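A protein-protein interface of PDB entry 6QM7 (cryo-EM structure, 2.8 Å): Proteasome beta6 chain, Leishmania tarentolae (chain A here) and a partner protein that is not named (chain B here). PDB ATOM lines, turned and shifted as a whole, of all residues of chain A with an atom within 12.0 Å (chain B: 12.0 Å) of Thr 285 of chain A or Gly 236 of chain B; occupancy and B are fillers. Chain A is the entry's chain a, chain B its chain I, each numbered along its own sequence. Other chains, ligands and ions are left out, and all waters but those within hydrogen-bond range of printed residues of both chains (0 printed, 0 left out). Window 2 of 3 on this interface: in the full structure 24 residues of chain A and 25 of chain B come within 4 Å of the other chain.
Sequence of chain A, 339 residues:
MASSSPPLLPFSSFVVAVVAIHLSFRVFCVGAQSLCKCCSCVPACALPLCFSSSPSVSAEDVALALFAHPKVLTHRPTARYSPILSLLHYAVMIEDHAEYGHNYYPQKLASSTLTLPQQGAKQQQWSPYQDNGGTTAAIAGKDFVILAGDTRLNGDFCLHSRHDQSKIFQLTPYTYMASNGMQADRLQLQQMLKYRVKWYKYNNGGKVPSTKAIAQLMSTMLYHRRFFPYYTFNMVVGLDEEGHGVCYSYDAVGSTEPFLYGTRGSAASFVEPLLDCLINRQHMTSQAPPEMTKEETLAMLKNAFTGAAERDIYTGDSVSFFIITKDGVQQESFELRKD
Thr 237 of chain B touches His 283 of chain A (O to O, 3.9 Å).
O of His 283 of chain A touches CA of Thr 238 of chain B (3.9 Å).
O of His 283 of chain A touches CD of Pro 239 of chain B, 3.7 Å away.
Met 284 of chain A touches Leu 233 of chain B.
Met 284 of chain A touches Thr 237 of chain B.
Gly 236 of chain B touches Thr 285 of chain A.
Pro 239 of chain B touches Thr 285 of chain A (CD to OG1, 3.9 Å).
O of Pro 234 of chain B lies within hydrogen-bond range of OG1 of Thr 237 of chain B.
The side-chain sulfur of Met 284 of chain A lies close to the guanidinium group of Arg 281 of chain A (3.6 Å).
OG1 of Thr 237 of chain B lies within hydrogen-bond range of OG of Ser 286 of chain A (3.0 Å).
The backbone carbonyl oxygen (O) of Thr 237 of chain B lies within hydrogen-bond range of the side-chain hydroxyl (OG1) of Thr 285 of chain A (2.7 Å).
Leu 278 of chain A touches none of the printed residues of chain B.
Of the printed residues of chain B, His 283 of chain A touches Thr 237, Thr 238 and Pro 239.
Of chain B, only Leu 233 and Thr 237 come within 4 Å of Met 284 of chain A.
Of chain B, only Gly 236, Thr 237 and Pro 239 come within 4 Å of Thr 285 of chain A.
Ser 286 of chain A touches just one residue of chain B: Thr 237.
No residue of chain B comes within 4 Å of Gln 287 of chain A.
Printed residues of chain A within 4 Å of Leu 233 of chain B: Met 284.
No residue of chain A comes within 4 Å of Pro 234 of chain B.
Pro 235 of chain B touches none of the printed residues of chain A.
Gly 236 of chain B touches just one residue of chain A: Thr 285 (3.5 Å).
Thr 237 of chain B touches just these residues of chain A: His 283, Met 284, Thr 285 and Ser 286.
Of chain A, only His 283 comes within 4 Å of Thr 238 of chain B.
The nearest residue of chain B that does not touch Thr 285 of chain A is Thr 238 of chain B (4.3 Å).
The nearest residue of chain A that does not touch Gly 236 of chain B is Ser 286 of chain A (5.4 Å).
Printed residues of chain B that touch a printed residue of chain A: Leu 233, Gly 236, Thr 237, Thr 238 and Pro 239.
Hydrophobic or aromatic side chains of chain B within 4 Å of the printed part of chain A: Leu 233 and Pro 239.
Among the printed residues, 9 pairs touch across the chains.
Among the printed residues, no Asp or Glu carboxylate lies within 4 Å of a Lys or Arg side-chain nitrogen of the other chain.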
ATOM      1  N   ASP A 276      -3.752  -0.811 -38.556  1.00  0.00           N
ATOM      2  CA  ASP A 276      -4.674  -1.948 -38.293  1.00  0.00           C
ATOM      3  C   ASP A 276      -5.268  -1.805 -36.888  1.00  0.00           C
ATOM      4  O   ASP A 276      -6.492  -1.915 -36.761  1.00  0.00           O
ATOM      5  CB  ASP A 276      -3.998  -3.326 -38.303  1.00  0.00           C
ATOM      6  CG  ASP A 276      -3.403  -3.836 -39.607  1.00  0.00           C
ATOM      7  OD1 ASP A 276      -3.729  -3.289 -40.683  1.00  0.00           O
ATOM      8  OD2 ASP A 276      -2.605  -4.803 -39.535  1.00  0.00           O
ATOM      9  N   CYS A 277      -4.426  -1.628 -35.865  1.00  0.00           N
ATOM     10  CA  CYS A 277      -4.831  -1.569 -34.435  1.00  0.00           C
ATOM     11  C   CYS A 277      -5.779  -0.390 -34.217  1.00  0.00           C
ATOM     12  O   CYS A 277      -6.832  -0.604 -33.616  1.00  0.00           O
ATOM     13  CB  CYS A 277      -3.630  -1.436 -33.501  1.00  0.00           C
ATOM     14  SG  CYS A 277      -4.019  -1.560 -31.728  1.00  0.00           S
ATOM     15  N   LEU A 278      -5.427   0.800 -34.701  1.00  0.00           N
ATOM     16  CA  LEU A 278      -6.090   2.067 -34.293  1.00  0.00           C
ATOM     17  C   LEU A 278      -7.304   2.370 -35.174  1.00  0.00           C
ATOM     18  O   LEU A 278      -8.136   3.180 -34.720  1.00  0.00           O
ATOM     19  CB  LEU A 278      -5.075   3.214 -34.343  1.00  0.00           C
ATOM     20  CG  LEU A 278      -3.889   3.094 -33.383  1.00  0.00           C
ATOM     21  CD1 LEU A 278      -3.085   4.385 -33.355  1.00  0.00           C
ATOM     22  CD2 LEU A 278      -4.332   2.698 -31.976  1.00  0.00           C
ATOM     23  N   ILE A 279      -7.413   1.752 -36.353  1.00  0.00           N
ATOM     24  CA  ILE A 279      -8.530   1.986 -37.310  1.00  0.00           C
ATOM     25  C   ILE A 279      -9.519   0.817 -37.239  1.00  0.00           C
ATOM     26  O   ILE A 279     -10.719   1.093 -37.031  1.00  0.00           O
ATOM     27  CB  ILE A 279      -7.977   2.221 -38.726  1.00  0.00           C
ATOM     28  CG1 ILE A 279      -7.134   3.497 -38.780  1.00  0.00           C
ATOM     29  CG2 ILE A 279      -9.087   2.241 -39.772  1.00  0.00           C
ATOM     30  CD1 ILE A 279      -6.231   3.582 -39.995  1.00  0.00           C
ATOM     31  N   ASN A 280      -9.044  -0.426 -37.391  1.00  0.00           N
ATOM     32  CA  ASN A 280      -9.895  -1.649 -37.462  1.00  0.00           C
ATOM     33  C   ASN A 280     -10.259  -2.159 -36.060  1.00  0.00           C
ATOM     34  O   ASN A 280     -11.315  -2.814 -35.947  1.00  0.00           O
ATOM     35  CB  ASN A 280      -9.248  -2.759 -38.297  1.00  0.00           C
ATOM     36  CG  ASN A 280      -9.187  -2.430 -39.774  1.00  0.00           C
ATOM     37  OD1 ASN A 280     -10.008  -1.668 -40.284  1.00  0.00           O
ATOM     38  ND2 ASN A 280      -8.226  -3.013 -40.476  1.00  0.00           N
ATOM     39  N   ARG A 281      -9.416  -1.910 -35.051  1.00  0.00           N
ATOM     40  CA  ARG A 281      -9.703  -2.153 -33.606  1.00  0.00           C
ATOM     41  C   ARG A 281     -10.159  -3.604 -33.362  1.00  0.00           C
ATOM     42  O   ARG A 281     -10.944  -3.814 -32.424  1.00  0.00           O
ATOM     43  CB  ARG A 281     -10.804  -1.211 -33.094  1.00  0.00           C
ATOM     44  CG  ARG A 281     -10.795   0.215 -33.632  1.00  0.00           C
ATOM     45  CD  ARG A 281     -10.051   1.204 -32.761  1.00  0.00           C
ATOM     46  NE  ARG A 281     -10.631   1.371 -31.433  1.00  0.00           N
ATOM     47  CZ  ARG A 281     -10.113   2.139 -30.471  1.00  0.00           C
ATOM     48  NH1 ARG A 281      -8.995   2.827 -30.675  1.00  0.00           N
ATOM     49  NH2 ARG A 281     -10.714   2.210 -29.294  1.00  0.00           N
ATOM     50  N   GLN A 282      -9.700  -4.580 -34.154  1.00  0.00           N
ATOM     51  CA  GLN A 282     -10.356  -5.918 -34.239  1.00  0.00           C
ATOM     52  C   GLN A 282     -10.142  -6.701 -32.934  1.00  0.00           C
ATOM     53  O   GLN A 282     -10.971  -7.585 -32.656  1.00  0.00           O
ATOM     54  CB  GLN A 282      -9.935  -6.675 -35.506  1.00  0.00           C
ATOM     55  CG  GLN A 282      -8.587  -7.382 -35.437  1.00  0.00           C
ATOM     56  CD  GLN A 282      -8.474  -8.549 -36.395  1.00  0.00           C
ATOM     57  OE1 GLN A 282      -9.260  -9.495 -36.361  1.00  0.00           O
ATOM     58  NE2 GLN A 282      -7.461  -8.504 -37.244  1.00  0.00           N
ATOM     59  N   HIS A 283      -9.124  -6.364 -32.135  1.00  0.00           N
ATOM     60  CA  HIS A 283      -8.856  -6.984 -30.806  1.00  0.00           C
ATOM     61  C   HIS A 283      -9.252  -6.044 -29.668  1.00  0.00           C
ATOM     62  O   HIS A 283      -8.540  -6.032 -28.646  1.00  0.00           O
ATOM     63  CB  HIS A 283      -7.385  -7.407 -30.695  1.00  0.00           C
ATOM     64  CG  HIS A 283      -7.035  -8.457 -31.684  1.00  0.00           C
ATOM     65  ND1 HIS A 283      -7.611  -9.710 -31.632  1.00  0.00           N
ATOM     66  CD2 HIS A 283      -6.241  -8.427 -32.773  1.00  0.00           C
ATOM     67  CE1 HIS A 283      -7.172 -10.419 -32.645  1.00  0.00           C
ATOM     68  NE2 HIS A 283      -6.325  -9.658 -33.352  1.00  0.00           N
ATOM     69  N   MET A 284     -10.356  -5.312 -29.822  1.00  0.00           N
ATOM     70  CA  MET A 284     -10.826  -4.338 -28.808  1.00  0.00           C
ATOM     71  C   MET A 284     -12.319  -4.543 -28.573  1.00  0.00           C
ATOM     72  O   MET A 284     -13.077  -4.576 -29.556  1.00  0.00           O
ATOM     73  CB  MET A 284     -10.520  -2.900 -29.230  1.00  0.00           C
ATOM     74  CG  MET A 284      -9.022  -2.614 -29.242  1.00  0.00           C
ATOM     75  SD  MET A 284      -8.603  -0.859 -29.415  1.00  0.00           S
ATOM     76  CE  MET A 284      -6.950  -0.961 -30.097  1.00  0.00           C
ATOM     77  N   THR A 285     -12.680  -4.709 -27.298  1.00  0.00           N
ATOM     78  CA  THR A 285     -14.054  -4.933 -26.783  1.00  0.00           C
ATOM     79  C   THR A 285     -14.794  -3.590 -26.719  1.00  0.00           C
ATOM     80  O   THR A 285     -16.026  -3.601 -26.884  1.00  0.00           O
ATOM     81  CB  THR A 285     -13.997  -5.646 -25.422  1.00  0.00           C
ATOM     82  OG1 THR A 285     -13.013  -6.680 -25.484  1.00  0.00           O
ATOM     83  CG2 THR A 285     -15.322  -6.249 -25.007  1.00  0.00           C
ATOM     84  N   SER A 286     -14.065  -2.487 -26.488  1.00  0.00           N
ATOM     85  CA  SER A 286     -14.551  -1.077 -26.502  1.00  0.00           C
ATOM     86  C   SER A 286     -15.363  -0.787 -27.774  1.00  0.00           C
ATOM     87  O   SER A 286     -15.045  -1.377 -28.830  1.00  0.00           O
ATOM     88  CB  SER A 286     -13.397  -0.102 -26.382  1.00  0.00           C
ATOM     89  OG  SER A 286     -12.458  -0.526 -25.401  1.00  0.00           O
ATOM     90  N   GLN A 287     -16.366   0.094 -27.669  1.00  0.00           N
ATOM     91  CA  GLN A 287     -17.190   0.585 -28.813  1.00  0.00           C
ATOM     92  C   GLN A 287     -16.303   1.458 -29.712  1.00  0.00           C
ATOM     93  O   GLN A 287     -15.610   2.341 -29.164  1.00  0.00           O
ATOM     94  CB  GLN A 287     -18.413   1.374 -28.323  1.00  0.00           C
ATOM     95  CG  GLN A 287     -19.467   0.524 -27.617  1.00  0.00           C
ATOM     96  CD  GLN A 287     -20.446  -0.140 -28.558  1.00  0.00           C
ATOM     97  OE1 GLN A 287     -20.121  -0.484 -29.693  1.00  0.00           O
ATOM     98  NE2 GLN A 287     -21.665  -0.338 -28.084  1.00  0.00           N
ATOM     99  N   ALA A 288     -16.322   1.211 -31.030  1.00  0.00           N
ATOM    100  CA  ALA A 288     -15.508   1.909 -32.058  1.00  0.00           C
ATOM    101  C   ALA A 288     -15.725   3.420 -31.949  1.00  0.00           C
ATOM    102  O   ALA A 288     -16.873   3.862 -31.952  1.00  0.00           O
ATOM    103  CB  ALA A 288     -15.868   1.399 -33.436  1.00  0.00           C
ATOM    104  N   PRO A 289     -14.658   4.256 -31.822  1.00  0.00           N
ATOM    105  CA  PRO A 289     -14.807   5.716 -31.820  1.00  0.00           C
ATOM    106  C   PRO A 289     -15.494   6.241 -33.084  1.00  0.00           C
ATOM    107  O   PRO A 289     -15.504   5.559 -34.109  1.00  0.00           O
ATOM    108  CB  PRO A 289     -13.364   6.243 -31.695  1.00  0.00           C
ATOM    109  CG  PRO A 289     -12.585   5.098 -31.092  1.00  0.00           C
ATOM    110  CD  PRO A 289     -13.254   3.849 -31.628  1.00  0.00           C
ATOM    111  N   LEU B 232      -5.475   5.713 -25.374  1.00  0.00           N
ATOM    112  CA  LEU B 232      -6.044   5.168 -24.109  1.00  0.00           C
ATOM    113  C   LEU B 232      -6.853   3.899 -24.412  1.00  0.00           C
ATOM    114  O   LEU B 232      -7.867   3.984 -25.137  1.00  0.00           O
ATOM    115  CB  LEU B 232      -6.882   6.231 -23.384  1.00  0.00           C
ATOM    116  CG  LEU B 232      -6.204   6.876 -22.168  1.00  0.00           C
ATOM    117  CD1 LEU B 232      -5.228   7.969 -22.592  1.00  0.00           C
ATOM    118  CD2 LEU B 232      -7.232   7.421 -21.182  1.00  0.00           C
ATOM    119  N   LEU B 233      -6.375   2.774 -23.868  1.00  0.00           N
ATOM    120  CA  LEU B 233      -6.986   1.423 -23.932  1.00  0.00           C
ATOM    121  C   LEU B 233      -7.391   1.022 -22.514  1.00  0.00           C
ATOM    122  O   LEU B 233      -6.577   0.484 -21.764  1.00  0.00           O
ATOM    123  CB  LEU B 233      -5.962   0.453 -24.534  1.00  0.00           C
ATOM    124  CG  LEU B 233      -5.389   0.857 -25.893  1.00  0.00           C
ATOM    125  CD1 LEU B 233      -4.309  -0.117 -26.346  1.00  0.00           C
ATOM    126  CD2 LEU B 233      -6.492   0.970 -26.939  1.00  0.00           C
ATOM    127  N   PRO B 234      -8.647   1.296 -22.084  1.00  0.00           N
ATOM    128  CA  PRO B 234      -9.052   1.037 -20.700  1.00  0.00           C
ATOM    129  C   PRO B 234      -9.084  -0.456 -20.377  1.00  0.00           C
ATOM    130  O   PRO B 234      -9.414  -1.259 -21.245  1.00  0.00           O
ATOM    131  CB  PRO B 234     -10.456   1.657 -20.611  1.00  0.00           C
ATOM    132  CG  PRO B 234     -10.968   1.615 -22.037  1.00  0.00           C
ATOM    133  CD  PRO B 234      -9.743   1.851 -22.896  1.00  0.00           C
ATOM    134  N   PRO B 235      -8.739  -0.879 -19.137  1.00  0.00           N
ATOM    135  CA  PRO B 235      -8.785  -2.295 -18.754  1.00  0.00           C
ATOM    136  C   PRO B 235     -10.049  -3.053 -19.199  1.00  0.00           C
ATOM    137  O   PRO B 235     -11.133  -2.500 -19.089  1.00  0.00           O
ATOM    138  CB  PRO B 235      -8.718  -2.228 -17.221  1.00  0.00           C
ATOM    139  CG  PRO B 235      -7.860  -1.005 -16.964  1.00  0.00           C
ATOM    140  CD  PRO B 235      -8.259  -0.020 -18.043  1.00  0.00           C
ATOM    141  N   GLY B 236      -9.872  -4.286 -19.698  1.00  0.00           N
ATOM    142  CA  GLY B 236     -10.937  -5.115 -20.300  1.00  0.00           C
ATOM    143  C   GLY B 236     -11.169  -4.793 -21.771  1.00  0.00           C
ATOM    144  O   GLY B 236     -12.153  -5.308 -22.340  1.00  0.00           O
ATOM    145  N   THR B 237     -10.304  -3.966 -22.369  1.00  0.00           N
ATOM    146  CA  THR B 237     -10.274  -3.663 -23.825  1.00  0.00           C
ATOM    147  C   THR B 237      -9.931  -4.947 -24.578  1.00  0.00           C
ATOM    148  O   THR B 237     -10.681  -5.299 -25.498  1.00  0.00           O
ATOM    149  CB  THR B 237      -9.301  -2.518 -24.139  1.00  0.00           C
ATOM    150  OG1 THR B 237     -10.022  -1.306 -23.915  1.00  0.00           O
ATOM    151  CG2 THR B 237      -8.769  -2.519 -25.557  1.00  0.00           C
ATOM    152  N   THR B 238      -8.840  -5.606 -24.189  1.00  0.00           N
ATOM    153  CA  THR B 238      -8.339  -6.855 -24.812  1.00  0.00           C
ATOM    154  C   THR B 238      -9.105  -8.033 -24.217  1.00  0.00           C
ATOM    155  O   THR B 238      -9.080  -8.209 -23.001  1.00  0.00           O
ATOM    156  CB  THR B 238      -6.826  -7.015 -24.615  1.00  0.00           C
ATOM    157  OG1 THR B 238      -6.170  -5.803 -24.995  1.00  0.00           O
ATOM    158  CG2 THR B 238      -6.259  -8.171 -25.410  1.00  0.00           C
ATOM    159  N   PRO B 239      -9.791  -8.863 -25.049  1.00  0.00           N
ATOM    160  CA  PRO B 239     -10.539 -10.023 -24.556  1.00  0.00           C
ATOM    161  C   PRO B 239      -9.634 -11.171 -24.078  1.00  0.00           C
ATOM    162  O   PRO B 239      -8.722 -11.546 -24.778  1.00  0.00           O
ATOM    163  CB  PRO B 239     -11.387 -10.459 -25.760  1.00  0.00           C
ATOM    164  CG  PRO B 239     -10.600  -9.990 -26.961  1.00  0.00           C
ATOM    165  CD  PRO B 239      -9.895  -8.728 -26.512  1.00  0.00           C
ATOM    166  N   VAL B 240      -9.943 -11.696 -22.891  1.00  0.00           N
ATOM    167  CA  VAL B 240      -9.105 -12.645 -22.107  1.00  0.00           C
ATOM    168  C   VAL B 240      -9.917 -13.921 -21.866  1.00  0.00           C
ATOM    169  O   VAL B 240     -10.987 -13.839 -21.239  1.00  0.00           O
ATOM    170  CB  VAL B 240      -8.655 -11.999 -20.783  1.00  0.00           C
ATOM    171  CG1 VAL B 240      -8.089 -13.017 -19.811  1.00  0.00           C
ATOM    172  CG2 VAL B 240      -7.651 -10.883 -21.012  1.00  0.00           C
ATOM    173  N   LEU B 241      -9.391 -15.056 -22.320  1.00  0.00           N
ATOM    174  CA  LEU B 241     -10.028 -16.387 -22.202  1.00  0.00           C
ATOM    175  C   LEU B 241      -9.863 -16.906 -20.772  1.00  0.00           C
ATOM    176  O   LEU B 241     -10.882 -17.284 -20.169  1.00  0.00           O
ATOM    177  CB  LEU B 241      -9.376 -17.332 -23.212  1.00  0.00           C
ATOM    178  CG  LEU B 241      -9.516 -16.920 -24.676  1.00  0.00           C
ATOM    179  CD1 LEU B 241      -8.731 -17.867 -25.578  1.00  0.00           C
ATOM    180  CD2 LEU B 241     -10.987 -16.861 -25.084  1.00  0.00           C
ATOM    181  N   LYS B 242      -8.631 -16.932 -20.262  1.00  0.00           N
ATOM    182  CA  LYS B 242      -8.290 -17.455 -18.911  1.00  0.00           C
ATOM    183  C   LYS B 242      -7.352 -16.483 -18.197  1.00  0.00           C
ATOM    184  O   LYS B 242      -6.692 -15.682 -18.875  1.00  0.00           O
ATOM    185  CB  LYS B 242      -7.639 -18.834 -19.013  1.00  0.00           C
ATOM    186  CG  LYS B 242      -8.612 -19.976 -19.258  1.00  0.00           C
ATOM    187  CD  LYS B 242      -7.948 -21.255 -19.724  1.00  0.00           C
ATOM    188  CE  LYS B 242      -8.769 -22.005 -20.754  1.00  0.00           C
ATOM    189  NZ  LYS B 242      -7.969 -23.055 -21.432  1.00  0.00           N
ATOM    190  N   GLU B 243      -7.310 -16.579 -16.871  1.00  0.00           N
ATOM    191  CA  GLU B 243      -6.540 -15.679 -15.980  1.00  0.00           C
ATOM    192  C   GLU B 243      -6.191 -16.453 -14.708  1.00  0.00           C
ATOM    193  O   GLU B 243      -7.131 -16.901 -14.033  1.00  0.00           O
ATOM    194  CB  GLU B 243      -7.372 -14.432 -15.685  1.00  0.00           C
ATOM    195  CG  GLU B 243      -6.694 -13.436 -14.754  1.00  0.00           C
ATOM    196  CD  GLU B 243      -7.436 -12.117 -14.566  1.00  0.00           C
ATOM    197  OE1 GLU B 243      -8.065 -11.634 -15.546  1.00  0.00           O
ATOM    198  OE2 GLU B 243      -7.374 -11.559 -13.447  1.00  0.00           O
